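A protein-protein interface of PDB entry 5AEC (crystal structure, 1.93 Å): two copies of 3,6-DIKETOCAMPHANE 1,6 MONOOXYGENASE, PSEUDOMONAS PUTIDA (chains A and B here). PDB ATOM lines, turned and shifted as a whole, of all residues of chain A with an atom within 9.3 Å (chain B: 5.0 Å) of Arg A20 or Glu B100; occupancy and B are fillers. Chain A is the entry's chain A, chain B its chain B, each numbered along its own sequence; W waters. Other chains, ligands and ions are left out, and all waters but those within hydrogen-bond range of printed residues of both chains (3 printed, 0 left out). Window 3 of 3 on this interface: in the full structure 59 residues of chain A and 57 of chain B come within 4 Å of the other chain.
Water W2 lies within hydrogen-bond range of OE1 of Gln B97 (2.8 Å) and N of Ala A19 (2.9 Å). Water W1 bridges the backbone carbonyl oxygen (O) of Gln B97 and the backbone NH (N) of Arg A20. Water W3 lies within hydrogen-bond range of the backbone carbonyl oxygen of Ile B98 (3.0 Å), the guanidinium group of Arg B102 (3.2 Å) and the guanidinium group of Arg A20 (3.5 Å).
Of the 9 printed residues of chain B, 4 touch a printed residue of chain A. Hydrophobic or aromatic side chains of chain B that line the printed part of chain A: Leu B66 and Ile B98. Of the 17 printed residues of chain A, 4 touch a printed residue of chain B. Hydrophobic or aromatic side chains of chain A within 4 Å of the printed part of chain B: Ala A19 and Phe A23. Among the printed residues, 7 pairs touch across the chains. Among the printed residues, no Asp or Glu carboxylate lies within 4 Å of a Lys or Arg side-chain nitrogen of the other chain.
No position is printed for both chains. Of the 7 pairs that touch across the chains among the printed residues, none has its exchanged pair printed and touching as well.
Among the printed residues, merely in contact across the chains: Ala A19 with Gln B97 (3.6 Å), Ala A19 with Ile B98 (3.97 Å), Arg A20 with Leu B66 (3.7 Å), Arg A20 with Ile B98 (3.8 Å), Arg A20 with Glu B100 (3.7 Å), Phe A23 with Ile B98 (3.5 Å) and Asp A24 with Leu B66 (3.7 Å).
Printed residues of chain B within 4 Å of Ala A19: Gln B97 and Ile B98. Of the printed residues of chain B, Arg A20 touches Leu B66 (3.7 Å), Ile B98 (3.8 Å) and Glu B100 (3.7 Å). Thr A22 touches none of the printed residues of chain B. Of the printed residues of chain A, Leu B66 touches Arg A20 (3.7 Å) and Asp A24 (3.7 Å). Of the printed residues of chain A, Ile B98 touches Ala A19, Arg A20 and Phe A23. Of the printed residues of chain A, Glu B100 touches Arg A20. Trp B191 touches none of the printed residues of chain A.
The side-chain amino group (NZ) of Lys A28 lies within salt-bridge range of the side-chain carboxylate (OD1) of Asp A24, 3.0 Å away. OH of Tyr A352 sits at hydrogen-bond distance from OD2 of Asp A24 (2.6 Å). The backbone carbonyl oxygen of Glu B100 sits at hydrogen-bond distance from the indole nitrogen of Trp B191, 3.4 Å away.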
ATOM      1  N   MET A  13      13.724 -14.038  12.317  1.00  0.00           N
ATOM      2  CA  MET A  13      13.684 -13.256  11.092  1.00  0.00           C
ATOM      3  C   MET A  13      14.520 -13.986  10.065  1.00  0.00           C
ATOM      4  O   MET A  13      15.619 -14.466  10.383  1.00  0.00           O
ATOM      5  CB  MET A  13      14.277 -11.847  11.274  1.00  0.00           C
ATOM      6  CG  MET A  13      13.501 -10.872  12.119  1.00  0.00           C
ATOM      7  SD  MET A  13      11.716 -10.751  11.862  1.00  0.00           S
ATOM      8  CE  MET A  13      11.539  -9.819  10.356  1.00  0.00           C
ATOM      9  N   GLY A  16      18.828 -11.877   6.080  1.00  0.00           N
ATOM     10  CA  GLY A  16      18.635 -10.850   5.063  1.00  0.00           C
ATOM     11  C   GLY A  16      17.660  -9.759   5.426  1.00  0.00           C
ATOM     12  O   GLY A  16      17.706  -8.684   4.830  1.00  0.00           O
ATOM     13  N   ARG A  17      16.757 -10.001   6.369  1.00  0.00           N
ATOM     14  CA  ARG A  17      15.955  -8.894   6.894  1.00  0.00           C
ATOM     15  C   ARG A  17      16.855  -7.829   7.496  1.00  0.00           C
ATOM     16  O   ARG A  17      17.818  -8.157   8.213  1.00  0.00           O
ATOM     17  CB  ARG A  17      15.028  -9.335   8.006  1.00  0.00           C
ATOM     18  CG  ARG A  17      14.032 -10.388   7.652  1.00  0.00           C
ATOM     19  CD  ARG A  17      13.147  -9.946   6.534  1.00  0.00           C
ATOM     20  NE  ARG A  17      11.878 -10.639   6.558  1.00  0.00           N
ATOM     21  CZ  ARG A  17      10.926 -10.431   5.644  1.00  0.00           C
ATOM     22  NH1 ARG A  17      11.090  -9.551   4.662  1.00  0.00           N
ATOM     23  NH2 ARG A  17       9.803 -11.098   5.736  1.00  0.00           N
ATOM     24  N   SER A  18      16.557  -6.568   7.207  1.00  0.00           N
ATOM     25  CA  SER A  18      17.264  -5.447   7.821  1.00  0.00           C
ATOM     26  C   SER A  18      16.821  -5.216   9.281  1.00  0.00           C
ATOM     27  O   SER A  18      15.795  -5.754   9.750  1.00  0.00           O
ATOM     28  CB  SER A  18      17.012  -4.166   7.051  1.00  0.00           C
ATOM     29  OG  SER A  18      15.670  -3.721   7.192  1.00  0.00           O
ATOM     30  N   ALA A  19      17.609  -4.422   9.979  1.00  0.00           N
ATOM     31  CA  ALA A  19      17.283  -3.986  11.346  1.00  0.00           C
ATOM     32  C   ALA A  19      15.971  -3.213  11.383  1.00  0.00           C
ATOM     33  O   ALA A  19      15.138  -3.480  12.257  1.00  0.00           O
ATOM     34  CB  ALA A  19      18.420  -3.150  11.916  1.00  0.00           C
ATOM     35  N   ARG A  20      15.763  -2.295  10.419  1.00  0.00           N
ATOM     36  CA  ARG A  20      14.523  -1.502  10.344  1.00  0.00           C
ATOM     37  C   ARG A  20      13.302  -2.393  10.119  1.00  0.00           C
ATOM     38  O   ARG A  20      12.269  -2.211  10.758  1.00  0.00           O
ATOM     39  CB  ARG A  20      14.586  -0.428   9.239  1.00  0.00           C
ATOM     40  CG  ARG A  20      13.348   0.466   9.224  1.00  0.00           C
ATOM     41  CD  ARG A  20      13.456   1.748   8.415  1.00  0.00           C
ATOM     42  NE  ARG A  20      12.209   2.532   8.525  1.00  0.00           N
ATOM     43  CZ  ARG A  20      11.019   2.210   8.016  1.00  0.00           C
ATOM     44  NH1 ARG A  20      10.834   1.117   7.278  1.00  0.00           N
ATOM     45  NH2 ARG A  20       9.989   3.010   8.241  1.00  0.00           N
ATOM     46  N   GLN A  21      13.418  -3.350   9.209  1.00  0.00           N
ATOM     47  CA  GLN A  21      12.330  -4.330   8.982  1.00  0.00           C
ATOM     48  C   GLN A  21      12.006  -5.152  10.237  1.00  0.00           C
ATOM     49  O   GLN A  21      10.840  -5.350  10.576  1.00  0.00           O
ATOM     50  CB  GLN A  21      12.687  -5.278   7.840  1.00  0.00           C
ATOM     51  CG  GLN A  21      12.635  -4.632   6.457  1.00  0.00           C
ATOM     52  CD  GLN A  21      13.153  -5.590   5.386  1.00  0.00           C
ATOM     53  OE1 GLN A  21      14.108  -6.327   5.610  1.00  0.00           O
ATOM     54  NE2 GLN A  21      12.532  -5.563   4.229  1.00  0.00           N
ATOM     55  N   THR A  22      13.043  -5.616  10.910  1.00  0.00           N
ATOM     56  CA  THR A  22      12.897  -6.398  12.133  1.00  0.00           C
ATOM     57  C   THR A  22      12.180  -5.577  13.205  1.00  0.00           C
ATOM     58  O   THR A  22      11.247  -6.073  13.833  1.00  0.00           O
ATOM     59  CB  THR A  22      14.256  -6.917  12.627  1.00  0.00           C
ATOM     60  OG1 THR A  22      14.852  -7.761  11.620  1.00  0.00           O
ATOM     61  CG2 THR A  22      14.114  -7.693  13.886  1.00  0.00           C
ATOM     62  N   PHE A  23      12.600  -4.333  13.369  1.00  0.00           N
ATOM     63  CA  PHE A  23      12.069  -3.420  14.379  1.00  0.00           C
ATOM     64  C   PHE A  23      10.621  -3.052  14.081  1.00  0.00           C
ATOM     65  O   PHE A  23       9.775  -3.006  14.986  1.00  0.00           O
ATOM     66  CB  PHE A  23      12.900  -2.143  14.417  1.00  0.00           C
ATOM     67  CG  PHE A  23      12.829  -1.403  15.735  1.00  0.00           C
ATOM     68  CD1 PHE A  23      13.490  -1.905  16.854  1.00  0.00           C
ATOM     69  CD2 PHE A  23      12.186  -0.183  15.843  1.00  0.00           C
ATOM     70  CE1 PHE A  23      13.444  -1.238  18.064  1.00  0.00           C
ATOM     71  CE2 PHE A  23      12.145   0.507  17.072  1.00  0.00           C
ATOM     72  CZ  PHE A  23      12.791  -0.025  18.173  1.00  0.00           C
ATOM     73  N   ASP A  24      10.359  -2.793  12.797  1.00  0.00           N
ATOM     74  CA  ASP A  24       8.987  -2.525  12.322  1.00  0.00           C
ATOM     75  C   ASP A  24       8.084  -3.734  12.582  1.00  0.00           C
ATOM     76  O   ASP A  24       6.996  -3.589  13.123  1.00  0.00           O
ATOM     77  CB  ASP A  24       9.039  -2.147  10.845  1.00  0.00           C
ATOM     78  CG  ASP A  24       7.726  -1.660  10.311  1.00  0.00           C
ATOM     79  OD1 ASP A  24       6.996  -0.933  11.020  1.00  0.00           O
ATOM     80  OD2 ASP A  24       7.444  -1.983   9.148  1.00  0.00           O
ATOM     81  N   TRP A  25       8.549  -4.944  12.276  1.00  0.00           N
ATOM     82  CA  TRP A  25       7.765  -6.152  12.563  1.00  0.00           C
ATOM     83  C   TRP A  25       7.481  -6.337  14.047  1.00  0.00           C
ATOM     84  O   TRP A  25       6.378  -6.800  14.413  1.00  0.00           O
ATOM     85  CB  TRP A  25       8.469  -7.383  12.015  1.00  0.00           C
ATOM     86  CG  TRP A  25       7.794  -8.668  12.214  1.00  0.00           C
ATOM     87  CD1 TRP A  25       8.364  -9.808  12.689  1.00  0.00           C
ATOM     88  CD2 TRP A  25       6.429  -8.998  11.911  1.00  0.00           C
ATOM     89  NE1 TRP A  25       7.446 -10.803  12.720  1.00  0.00           N
ATOM     90  CE2 TRP A  25       6.253 -10.334  12.236  1.00  0.00           C
ATOM     91  CE3 TRP A  25       5.342  -8.285  11.366  1.00  0.00           C
ATOM     92  CZ2 TRP A  25       5.035 -10.985  12.073  1.00  0.00           C
ATOM     93  CZ3 TRP A  25       4.137  -8.924  11.218  1.00  0.00           C
ATOM     94  CH2 TRP A  25       3.999 -10.264  11.548  1.00  0.00           C
ATOM     95  N   GLY A  26       8.473  -6.037  14.902  1.00  0.00           N
ATOM     96  CA  GLY A  26       8.273  -6.112  16.329  1.00  0.00           C
ATOM     97  C   GLY A  26       7.200  -5.165  16.852  1.00  0.00           C
ATOM     98  O   GLY A  26       6.382  -5.554  17.686  1.00  0.00           O
ATOM     99  N   ILE A  27       7.212  -3.924  16.367  1.00  0.00           N
ATOM    100  CA  ILE A  27       6.242  -2.914  16.809  1.00  0.00           C
ATOM    101  C   ILE A  27       4.860  -3.306  16.345  1.00  0.00           C
ATOM    102  O   ILE A  27       3.927  -3.316  17.138  1.00  0.00           O
ATOM    103  CB  ILE A  27       6.627  -1.478  16.355  1.00  0.00           C
ATOM    104  CG1 ILE A  27       7.921  -1.046  17.056  1.00  0.00           C
ATOM    105  CG2 ILE A  27       5.532  -0.476  16.740  1.00  0.00           C
ATOM    106  CD1 ILE A  27       8.542   0.173  16.441  1.00  0.00           C
ATOM    107  N   LYS A  28       4.750  -3.657  15.058  1.00  0.00           N
ATOM    108  CA  LYS A  28       3.492  -4.128  14.478  1.00  0.00           C
ATOM    109  C   LYS A  28       2.952  -5.343  15.228  1.00  0.00           C
ATOM    110  O   LYS A  28       1.746  -5.448  15.452  1.00  0.00           O
ATOM    111  CB  LYS A  28       3.671  -4.449  12.980  1.00  0.00           C
ATOM    112  CG  LYS A  28       3.742  -3.207  12.102  1.00  0.00           C
ATOM    113  CD  LYS A  28       4.046  -3.541  10.643  1.00  0.00           C
ATOM    114  CE  LYS A  28       3.583  -2.440   9.689  1.00  0.00           C
ATOM    115  NZ  LYS A  28       4.171  -1.094   9.957  1.00  0.00           N
ATOM    116  N   ASN A  53      17.772 -11.876  16.071  1.00  0.00           N
ATOM    117  CA  ASN A  53      18.560 -10.702  15.721  1.00  0.00           C
ATOM    118  C   ASN A  53      18.158  -9.423  16.477  1.00  0.00           C
ATOM    119  O   ASN A  53      18.235  -8.337  15.938  1.00  0.00           O
ATOM    120  CB  ASN A  53      18.490 -10.494  14.205  1.00  0.00           C
ATOM    121  CG  ASN A  53      17.078 -10.200  13.689  1.00  0.00           C
ATOM    122  OD1 ASN A  53      16.080 -10.396  14.400  1.00  0.00           O
ATOM    123  ND2 ASN A  53      16.994  -9.700  12.458  1.00  0.00           N
ATOM    124  N   LEU A  60      12.855  -2.187  21.580  1.00  0.00           N
ATOM    125  CA  LEU A  60      11.561  -2.548  21.024  1.00  0.00           C
ATOM    126  C   LEU A  60      10.432  -2.326  22.029  1.00  0.00           C
ATOM    127  O   LEU A  60       9.354  -1.799  21.688  1.00  0.00           O
ATOM    128  CB  LEU A  60      11.553  -4.007  20.554  1.00  0.00           C
ATOM    129  CG  LEU A  60      10.239  -4.576  19.996  1.00  0.00           C
ATOM    130  CD1 LEU A  60       9.625  -3.619  18.994  1.00  0.00           C
ATOM    131  CD2 LEU A  60      10.488  -5.933  19.346  1.00  0.00           C
ATOM    132  N   TYR A 352       6.325 -10.991   8.317  1.00  0.00           N
ATOM    133  CA  TYR A 352       6.381  -9.572   7.979  1.00  0.00           C
ATOM    134  C   TYR A 352       5.924  -9.283   6.575  1.00  0.00           C
ATOM    135  O   TYR A 352       5.381  -8.217   6.334  1.00  0.00           O
ATOM    136  CB  TYR A 352       7.818  -9.063   8.138  1.00  0.00           C
ATOM    137  CG  TYR A 352       8.049  -7.591   7.936  1.00  0.00           C
ATOM    138  CD1 TYR A 352       7.384  -6.647   8.715  1.00  0.00           C
ATOM    139  CD2 TYR A 352       8.943  -7.141   6.994  1.00  0.00           C
ATOM    140  CE1 TYR A 352       7.600  -5.285   8.544  1.00  0.00           C
ATOM    141  CE2 TYR A 352       9.155  -5.773   6.798  1.00  0.00           C
ATOM    142  CZ  TYR A 352       8.505  -4.855   7.612  1.00  0.00           C
ATOM    143  OH  TYR A 352       8.747  -3.499   7.482  1.00  0.00           O
ATOM    144  N   LEU B  66      11.001   5.304  13.812  1.00  0.00           N
ATOM    145  CA  LEU B  66      10.046   5.029  12.704  1.00  0.00           C
ATOM    146  C   LEU B  66       8.895   6.043  12.586  1.00  0.00           C
ATOM    147  O   LEU B  66       8.044   5.907  11.707  1.00  0.00           O
ATOM    148  CB  LEU B  66       9.449   3.614  12.823  1.00  0.00           C
ATOM    149  CG  LEU B  66      10.383   2.395  12.949  1.00  0.00           C
ATOM    150  CD1 LEU B  66       9.689   1.123  12.475  1.00  0.00           C
ATOM    151  CD2 LEU B  66      11.694   2.534  12.206  1.00  0.00           C
ATOM    152  N   SER B  96      21.750   2.580  14.955  1.00  0.00           N
ATOM    153  CA  SER B  96      22.201   3.251  13.740  1.00  0.00           C
ATOM    154  C   SER B  96      21.601   2.590  12.519  1.00  0.00           C
ATOM    155  O   SER B  96      21.129   3.272  11.609  1.00  0.00           O
ATOM    156  CB  SER B  96      23.740   3.220  13.652  1.00  0.00           C
ATOM    157  OG  SER B  96      24.212   3.647  12.380  1.00  0.00           O
ATOM    158  N   GLN B  97      21.578   1.260  12.498  1.00  0.00           N
ATOM    159  CA  GLN B  97      20.956   0.546  11.372  1.00  0.00           C
ATOM    160  C   GLN B  97      19.448   0.797  11.257  1.00  0.00           C
ATOM    161  O   GLN B  97      18.959   1.037  10.173  1.00  0.00           O
ATOM    162  CB  GLN B  97      21.187  -0.944  11.452  1.00  0.00           C
ATOM    163  CG  GLN B  97      22.596  -1.380  11.039  1.00  0.00           C
ATOM    164  CD  GLN B  97      22.710  -2.897  11.086  1.00  0.00           C
ATOM    165  OE1 GLN B  97      21.760  -3.611  10.736  1.00  0.00           O
ATOM    166  NE2 GLN B  97      23.841  -3.399  11.545  1.00  0.00           N
ATOM    167  N   ILE B  98      18.741   0.774  12.387  1.00  0.00           N
ATOM    168  CA  ILE B  98      17.289   1.012  12.446  1.00  0.00           C
ATOM    169  C   ILE B  98      16.989   2.392  11.874  1.00  0.00           C
ATOM    170  O   ILE B  98      16.009   2.561  11.145  1.00  0.00           O
ATOM    171  CB  ILE B  98      16.746   0.942  13.907  1.00  0.00           C
ATOM    172  CG1 ILE B  98      16.796  -0.497  14.452  1.00  0.00           C
ATOM    173  CG2 ILE B  98      15.302   1.452  13.990  1.00  0.00           C
ATOM    174  CD1 ILE B  98      16.652  -0.586  15.962  1.00  0.00           C
ATOM    175  N   LEU B  99      17.834   3.368  12.220  1.00  0.00           N
ATOM    176  CA  LEU B  99      17.703   4.734  11.728  1.00  0.00           C
ATOM    177  C   LEU B  99      18.239   4.981  10.315  1.00  0.00           C
ATOM    178  O   LEU B  99      18.185   6.117   9.854  1.00  0.00           O
ATOM    179  CB  LEU B  99      18.403   5.689  12.674  1.00  0.00           C
ATOM    180  CG  LEU B  99      17.644   5.969  13.978  1.00  0.00           C
ATOM    181  CD1 LEU B  99      18.599   6.536  15.020  1.00  0.00           C
ATOM    182  CD2 LEU B  99      16.515   6.928  13.741  1.00  0.00           C
ATOM    183  N   GLU B 100      18.808   3.962   9.675  1.00  0.00           N
ATOM    184  CA  GLU B 100      19.384   4.090   8.335  1.00  0.00           C
ATOM    185  C   GLU B 100      20.379   5.240   8.298  1.00  0.00           C
ATOM    186  O   GLU B 100      20.355   6.050   7.421  1.00  0.00           O
ATOM    187  CB  GLU B 100      18.284   4.222   7.295  1.00  0.00           C
ATOM    188  CG  GLU B 100      17.374   3.015   7.311  1.00  0.00           C
ATOM    189  CD  GLU B 100      16.248   3.108   6.293  1.00  0.00           C
ATOM    190  OE1 GLU B 100      15.693   4.196   6.052  1.00  0.00           O
ATOM    191  OE2 GLU B 100      15.959   2.078   5.697  1.00  0.00           O
ATOM    192  N   GLY B 101      21.210   5.323   9.336  1.00  0.00           N
ATOM    193  CA  GLY B 101      22.243   6.334   9.418  1.00  0.00           C
ATOM    194  C   GLY B 101      21.872   7.703   9.935  1.00  0.00           C
ATOM    195  O   GLY B 101      22.762   8.549  10.036  1.00  0.00           O
ATOM    196  N   ARG B 102      20.594   7.940  10.274  1.00  0.00           N
ATOM    197  CA  ARG B 102      20.157   9.201  10.877  1.00  0.00           C
ATOM    198  C   ARG B 102      20.529   9.217  12.367  1.00  0.00           C
ATOM    199  O   ARG B 102      19.690   9.395  13.240  1.00  0.00           O
ATOM    200  CB  ARG B 102      18.655   9.402  10.709  1.00  0.00           C
ATOM    201  CG  ARG B 102      18.198   9.471   9.265  1.00  0.00           C
ATOM    202  CD  ARG B 102      16.698   9.771   9.152  1.00  0.00           C
ATOM    203  NE  ARG B 102      15.856   8.661   9.601  1.00  0.00           N
ATOM    204  CZ  ARG B 102      14.942   8.688  10.583  1.00  0.00           C
ATOM    205  NH1 ARG B 102      14.669   9.775  11.286  1.00  0.00           N
ATOM    206  NH2 ARG B 102      14.269   7.578  10.849  1.00  0.00           N
ATOM    207  N   TRP B 191      25.586   1.861  10.512  1.00  0.00           N
ATOM    208  CA  TRP B 191      25.112   1.962   9.127  1.00  0.00           C
ATOM    209  C   TRP B 191      26.258   2.271   8.187  1.00  0.00           C
ATOM    210  O   TRP B 191      27.045   3.155   8.482  1.00  0.00           O
ATOM    211  CB  TRP B 191      24.108   3.088   9.049  1.00  0.00           C
ATOM    212  CG  TRP B 191      23.419   3.302   7.718  1.00  0.00           C
ATOM    213  CD1 TRP B 191      23.623   4.337   6.878  1.00  0.00           C
ATOM    214  CD2 TRP B 191      22.374   2.528   7.165  1.00  0.00           C
ATOM    215  NE1 TRP B 191      22.786   4.256   5.814  1.00  0.00           N
ATOM    216  CE2 TRP B 191      22.001   3.144   5.960  1.00  0.00           C
ATOM    217  CE3 TRP B 191      21.724   1.350   7.554  1.00  0.00           C
ATOM    218  CZ2 TRP B 191      21.005   2.630   5.141  1.00  0.00           C
ATOM    219  CZ3 TRP B 191      20.730   0.853   6.750  1.00  0.00           C
ATOM    220  CH2 TRP B 191      20.381   1.488   5.553  1.00  0.00           C
HETATM  221  O   HOH W   1      17.974  -1.146   8.592  1.00  0.00           O
HETATM  222  O   HOH W   2      19.942  -3.225   8.691  1.00  0.00           O
HETATM  223  O   HOH W   3      14.748   4.723   9.498  1.00  0.00           O
